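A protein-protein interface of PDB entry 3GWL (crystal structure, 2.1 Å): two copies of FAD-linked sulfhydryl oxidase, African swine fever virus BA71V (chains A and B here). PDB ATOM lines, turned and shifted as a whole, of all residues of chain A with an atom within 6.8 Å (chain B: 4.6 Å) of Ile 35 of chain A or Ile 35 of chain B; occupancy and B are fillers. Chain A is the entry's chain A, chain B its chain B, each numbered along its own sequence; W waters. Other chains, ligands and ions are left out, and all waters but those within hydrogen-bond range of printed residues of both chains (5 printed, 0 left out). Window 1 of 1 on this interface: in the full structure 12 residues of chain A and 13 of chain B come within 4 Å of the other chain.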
ATOM      1  N   TYR A  18      36.179  19.012  30.362  1.00  0.00           N
ATOM      2  CA  TYR A  18      35.664  19.067  29.001  1.00  0.00           C
ATOM      3  C   TYR A  18      34.301  19.759  29.056  1.00  0.00           C
ATOM      4  O   TYR A  18      33.968  20.583  28.204  1.00  0.00           O
ATOM      5  CB  TYR A  18      35.503  17.656  28.419  1.00  0.00           C
ATOM      6  CG  TYR A  18      35.041  17.642  26.975  1.00  0.00           C
ATOM      7  CD1 TYR A  18      35.937  17.855  25.927  1.00  0.00           C
ATOM      8  CD2 TYR A  18      33.700  17.434  26.662  1.00  0.00           C
ATOM      9  CE1 TYR A  18      35.503  17.859  24.594  1.00  0.00           C
ATOM     10  CE2 TYR A  18      33.256  17.436  25.348  1.00  0.00           C
ATOM     11  CZ  TYR A  18      34.155  17.648  24.319  1.00  0.00           C
ATOM     12  OH  TYR A  18      33.692  17.656  23.025  1.00  0.00           O
ATOM     13  N   GLU A  30      28.896  21.393  17.816  1.00  0.00           N
ATOM     14  CA  GLU A  30      29.643  21.183  19.049  1.00  0.00           C
ATOM     15  C   GLU A  30      28.924  20.170  19.940  1.00  0.00           C
ATOM     16  O   GLU A  30      29.564  19.393  20.655  1.00  0.00           O
ATOM     17  CB  GLU A  30      29.839  22.516  19.777  1.00  0.00           C
ATOM     18  CG  GLU A  30      30.424  23.595  18.873  1.00  0.00           C
ATOM     19  CD  GLU A  30      30.669  24.913  19.585  1.00  0.00           C
ATOM     20  OE1 GLU A  30      31.741  25.066  20.209  1.00  0.00           O
ATOM     21  OE2 GLU A  30      29.787  25.794  19.525  1.00  0.00           O
ATOM     22  N   LYS A  31      27.594  20.171  19.902  1.00  0.00           N
ATOM     23  CA  LYS A  31      26.842  19.211  20.702  1.00  0.00           C
ATOM     24  C   LYS A  31      27.124  17.808  20.169  1.00  0.00           C
ATOM     25  O   LYS A  31      27.309  16.865  20.935  1.00  0.00           O
ATOM     26  CB  LYS A  31      25.346  19.512  20.639  1.00  0.00           C
ATOM     27  CG  LYS A  31      24.953  20.811  21.316  1.00  0.00           C
ATOM     28  CD  LYS A  31      23.447  20.986  21.295  1.00  0.00           C
ATOM     29  CE  LYS A  31      23.034  22.339  21.829  1.00  0.00           C
ATOM     30  NZ  LYS A  31      21.560  22.515  21.692  1.00  0.00           N
ATOM     31  N   TYR A  32      27.171  17.686  18.847  1.00  0.00           N
ATOM     32  CA  TYR A  32      27.443  16.411  18.190  1.00  0.00           C
ATOM     33  C   TYR A  32      28.838  15.923  18.562  1.00  0.00           C
ATOM     34  O   TYR A  32      29.040  14.749  18.871  1.00  0.00           O
ATOM     35  CB  TYR A  32      27.368  16.569  16.668  1.00  0.00           C
ATOM     36  CG  TYR A  32      27.499  15.258  15.926  1.00  0.00           C
ATOM     37  CD1 TYR A  32      26.375  14.484  15.636  1.00  0.00           C
ATOM     38  CD2 TYR A  32      28.748  14.774  15.544  1.00  0.00           C
ATOM     39  CE1 TYR A  32      26.491  13.268  14.986  1.00  0.00           C
ATOM     40  CE2 TYR A  32      28.875  13.550  14.890  1.00  0.00           C
ATOM     41  CZ  TYR A  32      27.743  12.805  14.616  1.00  0.00           C
ATOM     42  OH  TYR A  32      27.859  11.591  13.978  1.00  0.00           O
ATOM     43  N   GLU A  33      29.805  16.833  18.520  1.00  0.00           N
ATOM     44  CA  GLU A  33      31.181  16.489  18.852  1.00  0.00           C
ATOM     45  C   GLU A  33      31.292  16.123  20.333  1.00  0.00           C
ATOM     46  O   GLU A  33      32.095  15.273  20.703  1.00  0.00           O
ATOM     47  CB  GLU A  33      32.103  17.662  18.499  1.00  0.00           C
ATOM     48  CG  GLU A  33      31.914  18.133  17.053  1.00  0.00           C
ATOM     49  CD  GLU A  33      32.915  19.191  16.620  1.00  0.00           C
ATOM     50  OE1 GLU A  33      33.089  20.192  17.347  1.00  0.00           O
ATOM     51  OE2 GLU A  33      33.520  19.023  15.542  1.00  0.00           O
ATOM     52  N   ALA A  34      30.476  16.751  21.174  1.00  0.00           N
ATOM     53  CA  ALA A  34      30.488  16.436  22.598  1.00  0.00           C
ATOM     54  C   ALA A  34      30.082  14.970  22.794  1.00  0.00           C
ATOM     55  O   ALA A  34      30.715  14.244  23.552  1.00  0.00           O
ATOM     56  CB  ALA A  34      29.535  17.353  23.350  1.00  0.00           C
ATOM     57  N   ILE A  35      29.037  14.531  22.097  1.00  0.00           N
ATOM     58  CA  ILE A  35      28.588  13.143  22.219  1.00  0.00           C
ATOM     59  C   ILE A  35      29.672  12.175  21.751  1.00  0.00           C
ATOM     60  O   ILE A  35      29.946  11.183  22.418  1.00  0.00           O
ATOM     61  CB  ILE A  35      27.274  12.891  21.424  1.00  0.00           C
ATOM     62  CG1 ILE A  35      26.131  13.682  22.059  1.00  0.00           C
ATOM     63  CG2 ILE A  35      26.928  11.398  21.418  1.00  0.00           C
ATOM     64  CD1 ILE A  35      24.771  13.389  21.454  1.00  0.00           C
ATOM     65  N   GLN A  36      30.301  12.454  20.612  1.00  0.00           N
ATOM     66  CA  GLN A  36      31.367  11.571  20.142  1.00  0.00           C
ATOM     67  C   GLN A  36      32.507  11.536  21.151  1.00  0.00           C
ATOM     68  O   GLN A  36      33.101  10.484  21.391  1.00  0.00           O
ATOM     69  CB  GLN A  36      31.924  12.038  18.798  1.00  0.00           C
ATOM     70  CG  GLN A  36      30.943  11.951  17.663  1.00  0.00           C
ATOM     71  CD  GLN A  36      31.628  12.025  16.319  1.00  0.00           C
ATOM     72  OE1 GLN A  36      31.315  11.077  15.445  1.00  0.00           O
ATOM     73  NE2 GLN A  36      32.429  12.923  16.069  1.00  0.00           N
ATOM     74  N   TRP A  37      32.810  12.688  21.742  1.00  0.00           N
ATOM     75  CA  TRP A  37      33.885  12.778  22.716  1.00  0.00           C
ATOM     76  C   TRP A  37      33.566  11.907  23.923  1.00  0.00           C
ATOM     77  O   TRP A  37      34.438  11.214  24.442  1.00  0.00           O
ATOM     78  CB  TRP A  37      34.084  14.235  23.172  1.00  0.00           C
ATOM     79  CG  TRP A  37      35.324  14.433  23.981  1.00  0.00           C
ATOM     80  CD1 TRP A  37      36.560  14.789  23.514  1.00  0.00           C
ATOM     81  CD2 TRP A  37      35.475  14.232  25.395  1.00  0.00           C
ATOM     82  NE1 TRP A  37      37.467  14.822  24.546  1.00  0.00           N
ATOM     83  CE2 TRP A  37      36.831  14.485  25.710  1.00  0.00           C
ATOM     84  CE3 TRP A  37      34.601  13.857  26.423  1.00  0.00           C
ATOM     85  CZ2 TRP A  37      37.334  14.377  27.014  1.00  0.00           C
ATOM     86  CZ3 TRP A  37      35.101  13.744  27.722  1.00  0.00           C
ATOM     87  CH2 TRP A  37      36.457  14.005  28.004  1.00  0.00           C
ATOM     88  N   ILE A  38      32.318  11.949  24.382  1.00  0.00           N
ATOM     89  CA  ILE A  38      31.927  11.140  25.529  1.00  0.00           C
ATOM     90  C   ILE A  38      32.075   9.658  25.186  1.00  0.00           C
ATOM     91  O   ILE A  38      32.553   8.872  26.000  1.00  0.00           O
ATOM     92  CB  ILE A  38      30.472  11.442  25.968  1.00  0.00           C
ATOM     93  CG1 ILE A  38      30.405  12.840  26.596  1.00  0.00           C
ATOM     94  CG2 ILE A  38      29.990  10.386  26.973  1.00  0.00           C
ATOM     95  CD1 ILE A  38      31.213  12.990  27.901  1.00  0.00           C
ATOM     96  N   LEU A  39      31.676   9.278  23.976  1.00  0.00           N
ATOM     97  CA  LEU A  39      31.793   7.883  23.559  1.00  0.00           C
ATOM     98  C   LEU A  39      33.268   7.459  23.525  1.00  0.00           C
ATOM     99  O   LEU A  39      33.615   6.349  23.918  1.00  0.00           O
ATOM    100  CB  LEU A  39      31.148   7.684  22.183  1.00  0.00           C
ATOM    101  CG  LEU A  39      29.625   7.859  22.159  1.00  0.00           C
ATOM    102  CD1 LEU A  39      29.119   7.775  20.729  1.00  0.00           C
ATOM    103  CD2 LEU A  39      28.967   6.783  23.025  1.00  0.00           C
ATOM    104  N   ASN A  40      34.133   8.351  23.057  1.00  0.00           N
ATOM    105  CA  ASN A  40      35.557   8.050  22.996  1.00  0.00           C
ATOM    106  C   ASN A  40      36.152   8.042  24.402  1.00  0.00           C
ATOM    107  O   ASN A  40      37.085   7.292  24.689  1.00  0.00           O
ATOM    108  CB  ASN A  40      36.272   9.066  22.109  1.00  0.00           C
ATOM    109  CG  ASN A  40      35.876   8.935  20.650  1.00  0.00           C
ATOM    110  OD1 ASN A  40      35.756   7.824  20.129  1.00  0.00           O
ATOM    111  ND2 ASN A  40      35.683  10.066  19.979  1.00  0.00           N
ATOM    112  N   PHE A  41      35.593   8.862  25.283  1.00  0.00           N
ATOM    113  CA  PHE A  41      36.065   8.916  26.662  1.00  0.00           C
ATOM    114  C   PHE A  41      35.795   7.580  27.353  1.00  0.00           C
ATOM    115  O   PHE A  41      36.657   7.039  28.051  1.00  0.00           O
ATOM    116  CB  PHE A  41      35.355  10.044  27.414  1.00  0.00           C
ATOM    117  CG  PHE A  41      35.562  10.009  28.899  1.00  0.00           C
ATOM    118  CD1 PHE A  41      36.762  10.443  29.464  1.00  0.00           C
ATOM    119  CD2 PHE A  41      34.560   9.532  29.737  1.00  0.00           C
ATOM    120  CE1 PHE A  41      36.954  10.407  30.844  1.00  0.00           C
ATOM    121  CE2 PHE A  41      34.738   9.486  31.124  1.00  0.00           C
ATOM    122  CZ  PHE A  41      35.939   9.925  31.682  1.00  0.00           C
ATOM    123  N   LEU A  58      24.996   6.169  30.318  1.00  0.00           N
ATOM    124  CA  LEU A  58      24.773   7.114  29.229  1.00  0.00           C
ATOM    125  C   LEU A  58      23.452   6.901  28.489  1.00  0.00           C
ATOM    126  O   LEU A  58      22.714   7.858  28.250  1.00  0.00           O
ATOM    127  CB  LEU A  58      25.928   7.057  28.229  1.00  0.00           C
ATOM    128  CG  LEU A  58      25.758   7.916  26.974  1.00  0.00           C
ATOM    129  CD1 LEU A  58      25.584   9.374  27.357  1.00  0.00           C
ATOM    130  CD2 LEU A  58      26.972   7.734  26.076  1.00  0.00           C
ATOM    131  N   LEU A  63      22.734  12.858  27.411  1.00  0.00           N
ATOM    132  CA  LEU A  63      23.555  14.025  27.688  1.00  0.00           C
ATOM    133  C   LEU A  63      22.699  15.283  27.622  1.00  0.00           C
ATOM    134  O   LEU A  63      21.816  15.402  26.774  1.00  0.00           O
ATOM    135  CB  LEU A  63      24.706  14.107  26.676  1.00  0.00           C
ATOM    136  CG  LEU A  63      25.808  13.065  26.891  1.00  0.00           C
ATOM    137  CD1 LEU A  63      26.685  12.932  25.657  1.00  0.00           C
ATOM    138  CD2 LEU A  63      26.630  13.473  28.115  1.00  0.00           C
ATOM    139  N   LEU A  65      23.177  18.891  26.869  1.00  0.00           N
ATOM    140  CA  LEU A  65      24.138  19.801  26.263  1.00  0.00           C
ATOM    141  C   LEU A  65      23.663  21.186  25.819  1.00  0.00           C
ATOM    142  O   LEU A  65      24.192  21.735  24.846  1.00  0.00           O
ATOM    143  CB  LEU A  65      24.783  19.090  25.072  1.00  0.00           C
ATOM    144  CG  LEU A  65      25.274  17.666  25.355  1.00  0.00           C
ATOM    145  CD1 LEU A  65      25.607  16.961  24.051  1.00  0.00           C
ATOM    146  CD2 LEU A  65      26.490  17.720  26.276  1.00  0.00           C
ATOM    147  N   PHE A  71      25.952  20.598  31.008  1.00  0.00           N
ATOM    148  CA  PHE A  71      26.857  19.498  30.704  1.00  0.00           C
ATOM    149  C   PHE A  71      27.647  19.185  31.981  1.00  0.00           C
ATOM    150  O   PHE A  71      27.840  18.021  32.331  1.00  0.00           O
ATOM    151  CB  PHE A  71      27.783  19.919  29.558  1.00  0.00           C
ATOM    152  CG  PHE A  71      28.590  18.794  28.954  1.00  0.00           C
ATOM    153  CD1 PHE A  71      28.468  17.487  29.405  1.00  0.00           C
ATOM    154  CD2 PHE A  71      29.492  19.060  27.927  1.00  0.00           C
ATOM    155  CE1 PHE A  71      29.239  16.458  28.842  1.00  0.00           C
ATOM    156  CE2 PHE A  71      30.260  18.043  27.363  1.00  0.00           C
ATOM    157  CZ  PHE A  71      30.135  16.739  27.821  1.00  0.00           C
ATOM    158  N   LYS B  31      21.938  15.541  12.412  1.00  0.00           N
ATOM    159  CA  LYS B  31      23.009  14.593  12.680  1.00  0.00           C
ATOM    160  C   LYS B  31      23.024  14.327  14.184  1.00  0.00           C
ATOM    161  O   LYS B  31      23.171  13.187  14.630  1.00  0.00           O
ATOM    162  CB  LYS B  31      24.351  15.173  12.223  1.00  0.00           C
ATOM    163  CG  LYS B  31      24.450  15.359  10.716  1.00  0.00           C
ATOM    164  CD  LYS B  31      25.813  15.916  10.292  1.00  0.00           C
ATOM    165  CE  LYS B  31      25.868  16.110   8.780  1.00  0.00           C
ATOM    166  NZ  LYS B  31      27.164  16.678   8.312  1.00  0.00           N
ATOM    167  N   TYR B  32      22.851  15.386  14.964  1.00  0.00           N
ATOM    168  CA  TYR B  32      22.830  15.262  16.409  1.00  0.00           C
ATOM    169  C   TYR B  32      21.658  14.388  16.873  1.00  0.00           C
ATOM    170  O   TYR B  32      21.807  13.541  17.754  1.00  0.00           O
ATOM    171  CB  TYR B  32      22.718  16.643  17.057  1.00  0.00           C
ATOM    172  CG  TYR B  32      22.539  16.575  18.551  1.00  0.00           C
ATOM    173  CD1 TYR B  32      23.627  16.380  19.392  1.00  0.00           C
ATOM    174  CD2 TYR B  32      21.272  16.668  19.124  1.00  0.00           C
ATOM    175  CE1 TYR B  32      23.462  16.282  20.770  1.00  0.00           C
ATOM    176  CE2 TYR B  32      21.098  16.569  20.504  1.00  0.00           C
ATOM    177  CZ  TYR B  32      22.199  16.377  21.317  1.00  0.00           C
ATOM    178  OH  TYR B  32      22.043  16.302  22.678  1.00  0.00           O
ATOM    179  N   GLU B  33      20.491  14.600  16.281  1.00  0.00           N
ATOM    180  CA  GLU B  33      19.311  13.824  16.649  1.00  0.00           C
ATOM    181  C   GLU B  33      19.458  12.378  16.183  1.00  0.00           C
ATOM    182  O   GLU B  33      18.900  11.463  16.784  1.00  0.00           O
ATOM    183  CB  GLU B  33      18.058  14.468  16.042  1.00  0.00           C
ATOM    184  CG  GLU B  33      17.853  15.912  16.502  1.00  0.00           C
ATOM    185  CD  GLU B  33      16.777  16.649  15.722  1.00  0.00           C
ATOM    186  OE1 GLU B  33      16.736  16.504  14.483  1.00  0.00           O
ATOM    187  OE2 GLU B  33      15.985  17.391  16.345  1.00  0.00           O
ATOM    188  N   ALA B  34      20.236  12.179  15.121  1.00  0.00           N
ATOM    189  CA  ALA B  34      20.466  10.845  14.579  1.00  0.00           C
ATOM    190  C   ALA B  34      21.350  10.031  15.514  1.00  0.00           C
ATOM    191  O   ALA B  34      21.072   8.863  15.771  1.00  0.00           O
ATOM    192  CB  ALA B  34      21.110  10.940  13.195  1.00  0.00           C
ATOM    193  N   ILE B  35      22.416  10.641  16.027  1.00  0.00           N
ATOM    194  CA  ILE B  35      23.294   9.915  16.927  1.00  0.00           C
ATOM    195  C   ILE B  35      22.597   9.655  18.261  1.00  0.00           C
ATOM    196  O   ILE B  35      22.831   8.626  18.893  1.00  0.00           O
ATOM    197  CB  ILE B  35      24.635  10.666  17.156  1.00  0.00           C
ATOM    198  CG1 ILE B  35      25.607   9.765  17.917  1.00  0.00           C
ATOM    199  CG2 ILE B  35      24.402  11.953  17.927  1.00  0.00           C
ATOM    200  CD1 ILE B  35      27.017  10.327  18.018  1.00  0.00           C
ATOM    201  N   GLN B  36      21.728  10.571  18.688  1.00  0.00           N
ATOM    202  CA  GLN B  36      21.014  10.374  19.945  1.00  0.00           C
ATOM    203  C   GLN B  36      20.000   9.246  19.763  1.00  0.00           C
ATOM    204  O   GLN B  36      19.781   8.438  20.673  1.00  0.00           O
ATOM    205  CB  GLN B  36      20.303  11.661  20.377  1.00  0.00           C
ATOM    206  CG  GLN B  36      19.660  11.576  21.761  1.00  0.00           C
ATOM    207  CD  GLN B  36      20.657  11.210  22.855  1.00  0.00           C
ATOM    208  OE1 GLN B  36      21.614  11.940  23.109  1.00  0.00           O
ATOM    209  NE2 GLN B  36      20.429  10.070  23.510  1.00  0.00           N
ATOM    210  N   TRP B  37      19.389   9.193  18.583  1.00  0.00           N
ATOM    211  CA  TRP B  37      18.417   8.150  18.263  1.00  0.00           C
ATOM    212  C   TRP B  37      19.088   6.781  18.328  1.00  0.00           C
ATOM    213  O   TRP B  37      18.484   5.807  18.779  1.00  0.00           O
ATOM    214  CB  TRP B  37      17.857   8.343  16.853  1.00  0.00           C
ATOM    215  CG  TRP B  37      16.697   7.439  16.536  1.00  0.00           C
ATOM    216  CD1 TRP B  37      15.375   7.706  16.734  1.00  0.00           C
ATOM    217  CD2 TRP B  37      16.756   6.124  15.961  1.00  0.00           C
ATOM    218  NE1 TRP B  37      14.605   6.646  16.317  1.00  0.00           N
ATOM    219  CE2 TRP B  37      15.427   5.661  15.839  1.00  0.00           C
ATOM    220  CE3 TRP B  37      17.804   5.292  15.539  1.00  0.00           C
ATOM    221  CZ2 TRP B  37      15.114   4.402  15.309  1.00  0.00           C
ATOM    222  CZ3 TRP B  37      17.496   4.041  15.014  1.00  0.00           C
ATOM    223  CH2 TRP B  37      16.161   3.608  14.903  1.00  0.00           C
ATOM    224  N   ILE B  38      20.340   6.718  17.866  1.00  0.00           N
ATOM    225  CA  ILE B  38      21.107   5.475  17.861  1.00  0.00           C
ATOM    226  C   ILE B  38      21.363   5.002  19.281  1.00  0.00           C
ATOM    227  O   ILE B  38      21.167   3.824  19.590  1.00  0.00           O
ATOM    228  CB  ILE B  38      22.458   5.649  17.116  1.00  0.00           C
ATOM    229  CG1 ILE B  38      22.209   5.799  15.611  1.00  0.00           C
ATOM    230  CG2 ILE B  38      23.375   4.466  17.389  1.00  0.00           C
ATOM    231  CD1 ILE B  38      21.680   4.532  14.925  1.00  0.00           C
ATOM    232  N   LEU B  39      21.799   5.912  20.150  1.00  0.00           N
ATOM    233  CA  LEU B  39      22.037   5.543  21.540  1.00  0.00           C
ATOM    234  C   LEU B  39      20.724   5.054  22.150  1.00  0.00           C
ATOM    235  O   LEU B  39      20.700   4.061  22.870  1.00  0.00           O
ATOM    236  CB  LEU B  39      22.585   6.734  22.338  1.00  0.00           C
ATOM    237  CG  LEU B  39      24.000   7.186  21.941  1.00  0.00           C
ATOM    238  CD1 LEU B  39      24.355   8.469  22.663  1.00  0.00           C
ATOM    239  CD2 LEU B  39      25.002   6.089  22.269  1.00  0.00           C
ATOM    240  N   LEU B  63      29.546   7.040  13.344  1.00  0.00           N
ATOM    241  CA  LEU B  63      28.445   7.160  12.397  1.00  0.00           C
ATOM    242  C   LEU B  63      28.843   8.007  11.186  1.00  0.00           C
ATOM    243  O   LEU B  63      29.529   9.019  11.325  1.00  0.00           O
ATOM    244  CB  LEU B  63      27.237   7.822  13.068  1.00  0.00           C
ATOM    245  CG  LEU B  63      26.434   7.038  14.105  1.00  0.00           C
ATOM    246  CD1 LEU B  63      25.392   7.958  14.722  1.00  0.00           C
ATOM    247  CD2 LEU B  63      25.769   5.832  13.444  1.00  0.00           C
HETATM  248  O   HOH W   1      21.723  14.424  24.187  1.00  0.00           O
HETATM  249  O   HOH W   2      23.246  11.430  25.202  1.00  0.00           O
HETATM  250  O   HOH W   3      22.417   8.622  25.696  1.00  0.00           O
HETATM  251  O   HOH W   4      20.943  18.218  24.491  1.00  0.00           O
HETATM  252  O   HOH W   5      30.054  10.398  13.425  1.00  0.00           O
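Lys 31 of chain A touches Tyr 32 of chain B, and with the chains exchanged Tyr 32 of chain A touches Lys 31 of chain B.
Tyr 32 of chain A touches its own counterpart, Tyr 32 of chain B.
Tyr 32 of chain A touches Leu 63 of chain B, but with the chains exchanged Leu 63 of chain A does not touch Tyr 32 of chain B (4.2 Å).
Ile 35 of chain A touches its own counterpart, Ile 35 of chain B.
Positions printed for both chains: 31, 32, 33, 34, 35, 36, 37, 38, 39 and 63.
CB of Lys 31 of chain A touches CE1 of Tyr 32 of chain B (3.7 Å).
Tyr 32 of chain A touches Lys 31 of chain B (CE1 to O, 3.3 Å).
Tyr 32 of chain B touches Tyr 32 of chain A.
Tyr 32 of chain A touches Ile 35 of chain B (CE1 to CG2, 3.8 Å).
Tyr 32 of chain A touches Leu 63 of chain B.
CE1 of Tyr 32 of chain B touches CD1 of Ile 35 of chain A (3.2 Å).
Ile 35 of chain B touches Ile 35 of chain A (CD1 to CG2, 3.6 Å).
Gln 36 of chain B touches Ile 35 of chain A.
Leu 65 of chain A touches Tyr 32 of chain B.
Of the printed residues of chain B, Lys 31 of chain A touches Tyr 32 (3.7 Å).
Printed residues of chain B within 4 Å of Tyr 32 of chain A: Lys 31, Tyr 32, Ile 35 and Leu 63.
Of chain B, only Tyr 32 (3.2 Å), Ile 35 (3.6 Å) and Gln 36 (3.8 Å) come within 4 Å of Ile 35 of chain A.
Of the printed residues of chain B, Leu 65 of chain A touches Tyr 32 (3.9 Å).
Of the printed residues of chain A, Tyr 32 of chain B touches Lys 31, Tyr 32, Ile 35 and Leu 65.
Glu 33 of chain B touches none of the printed residues of chain A.
Of chain A, only Tyr 32 and Ile 35 come within 4 Å of Ile 35 of chain B.
Printed residues of chain A within 4 Å of Leu 63 of chain B: Tyr 32 (3.9 Å).
The nearest residue of chain B that does not touch Ile 35 of chain A is Leu 39 of chain B (4.1 Å).
The nearest printed residue of chain A that does not touch Ile 35 of chain B is Gln 36 of chain A (4.3 Å).
Water W1 lies within hydrogen-bond range of OH of Tyr 32 of chain B (2.4 Å), OE1 of Gln 36 of chain B (2.7 Å) and O of Leu 63 of chain A (2.8 Å).
Water W5 lies within hydrogen-bond range of the side-chain amide oxygen (OE1) of Gln 36 of chain A, the side-chain hydroxyl (OH) of Tyr 32 of chain A and the backbone carbonyl oxygen (O) of Leu 63 of chain B.
Water W2 lies within hydrogen-bond range of the backbone NH of Leu 63 of chain A (2.7 Å) and the side-chain amide oxygen of Gln 36 of chain B (2.7 Å).
Water W3 lies within hydrogen-bond range of the backbone carbonyl oxygen (O) of Leu 58 of chain A and the side-chain amide nitrogen (NE2) of Gln 36 of chain B.
Water W4 lies within hydrogen-bond range of OH of Tyr 32 of chain B (2.9 Å) and N of Leu 65 of chain A (3.3 Å).
Printed residues of chain B that touch a printed residue of chain A: Lys 31, Tyr 32, Ile 35, Gln 36 and Leu 63.
Of the 17 printed residues of chain A, 4 touch a printed residue of chain B.
Among the printed residues, 9 pairs touch across the chains.
Among the printed residues, no Asp or Glu carboxylate lies within 4 Å of a Lys or Arg side-chain nitrogen of the other chain.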
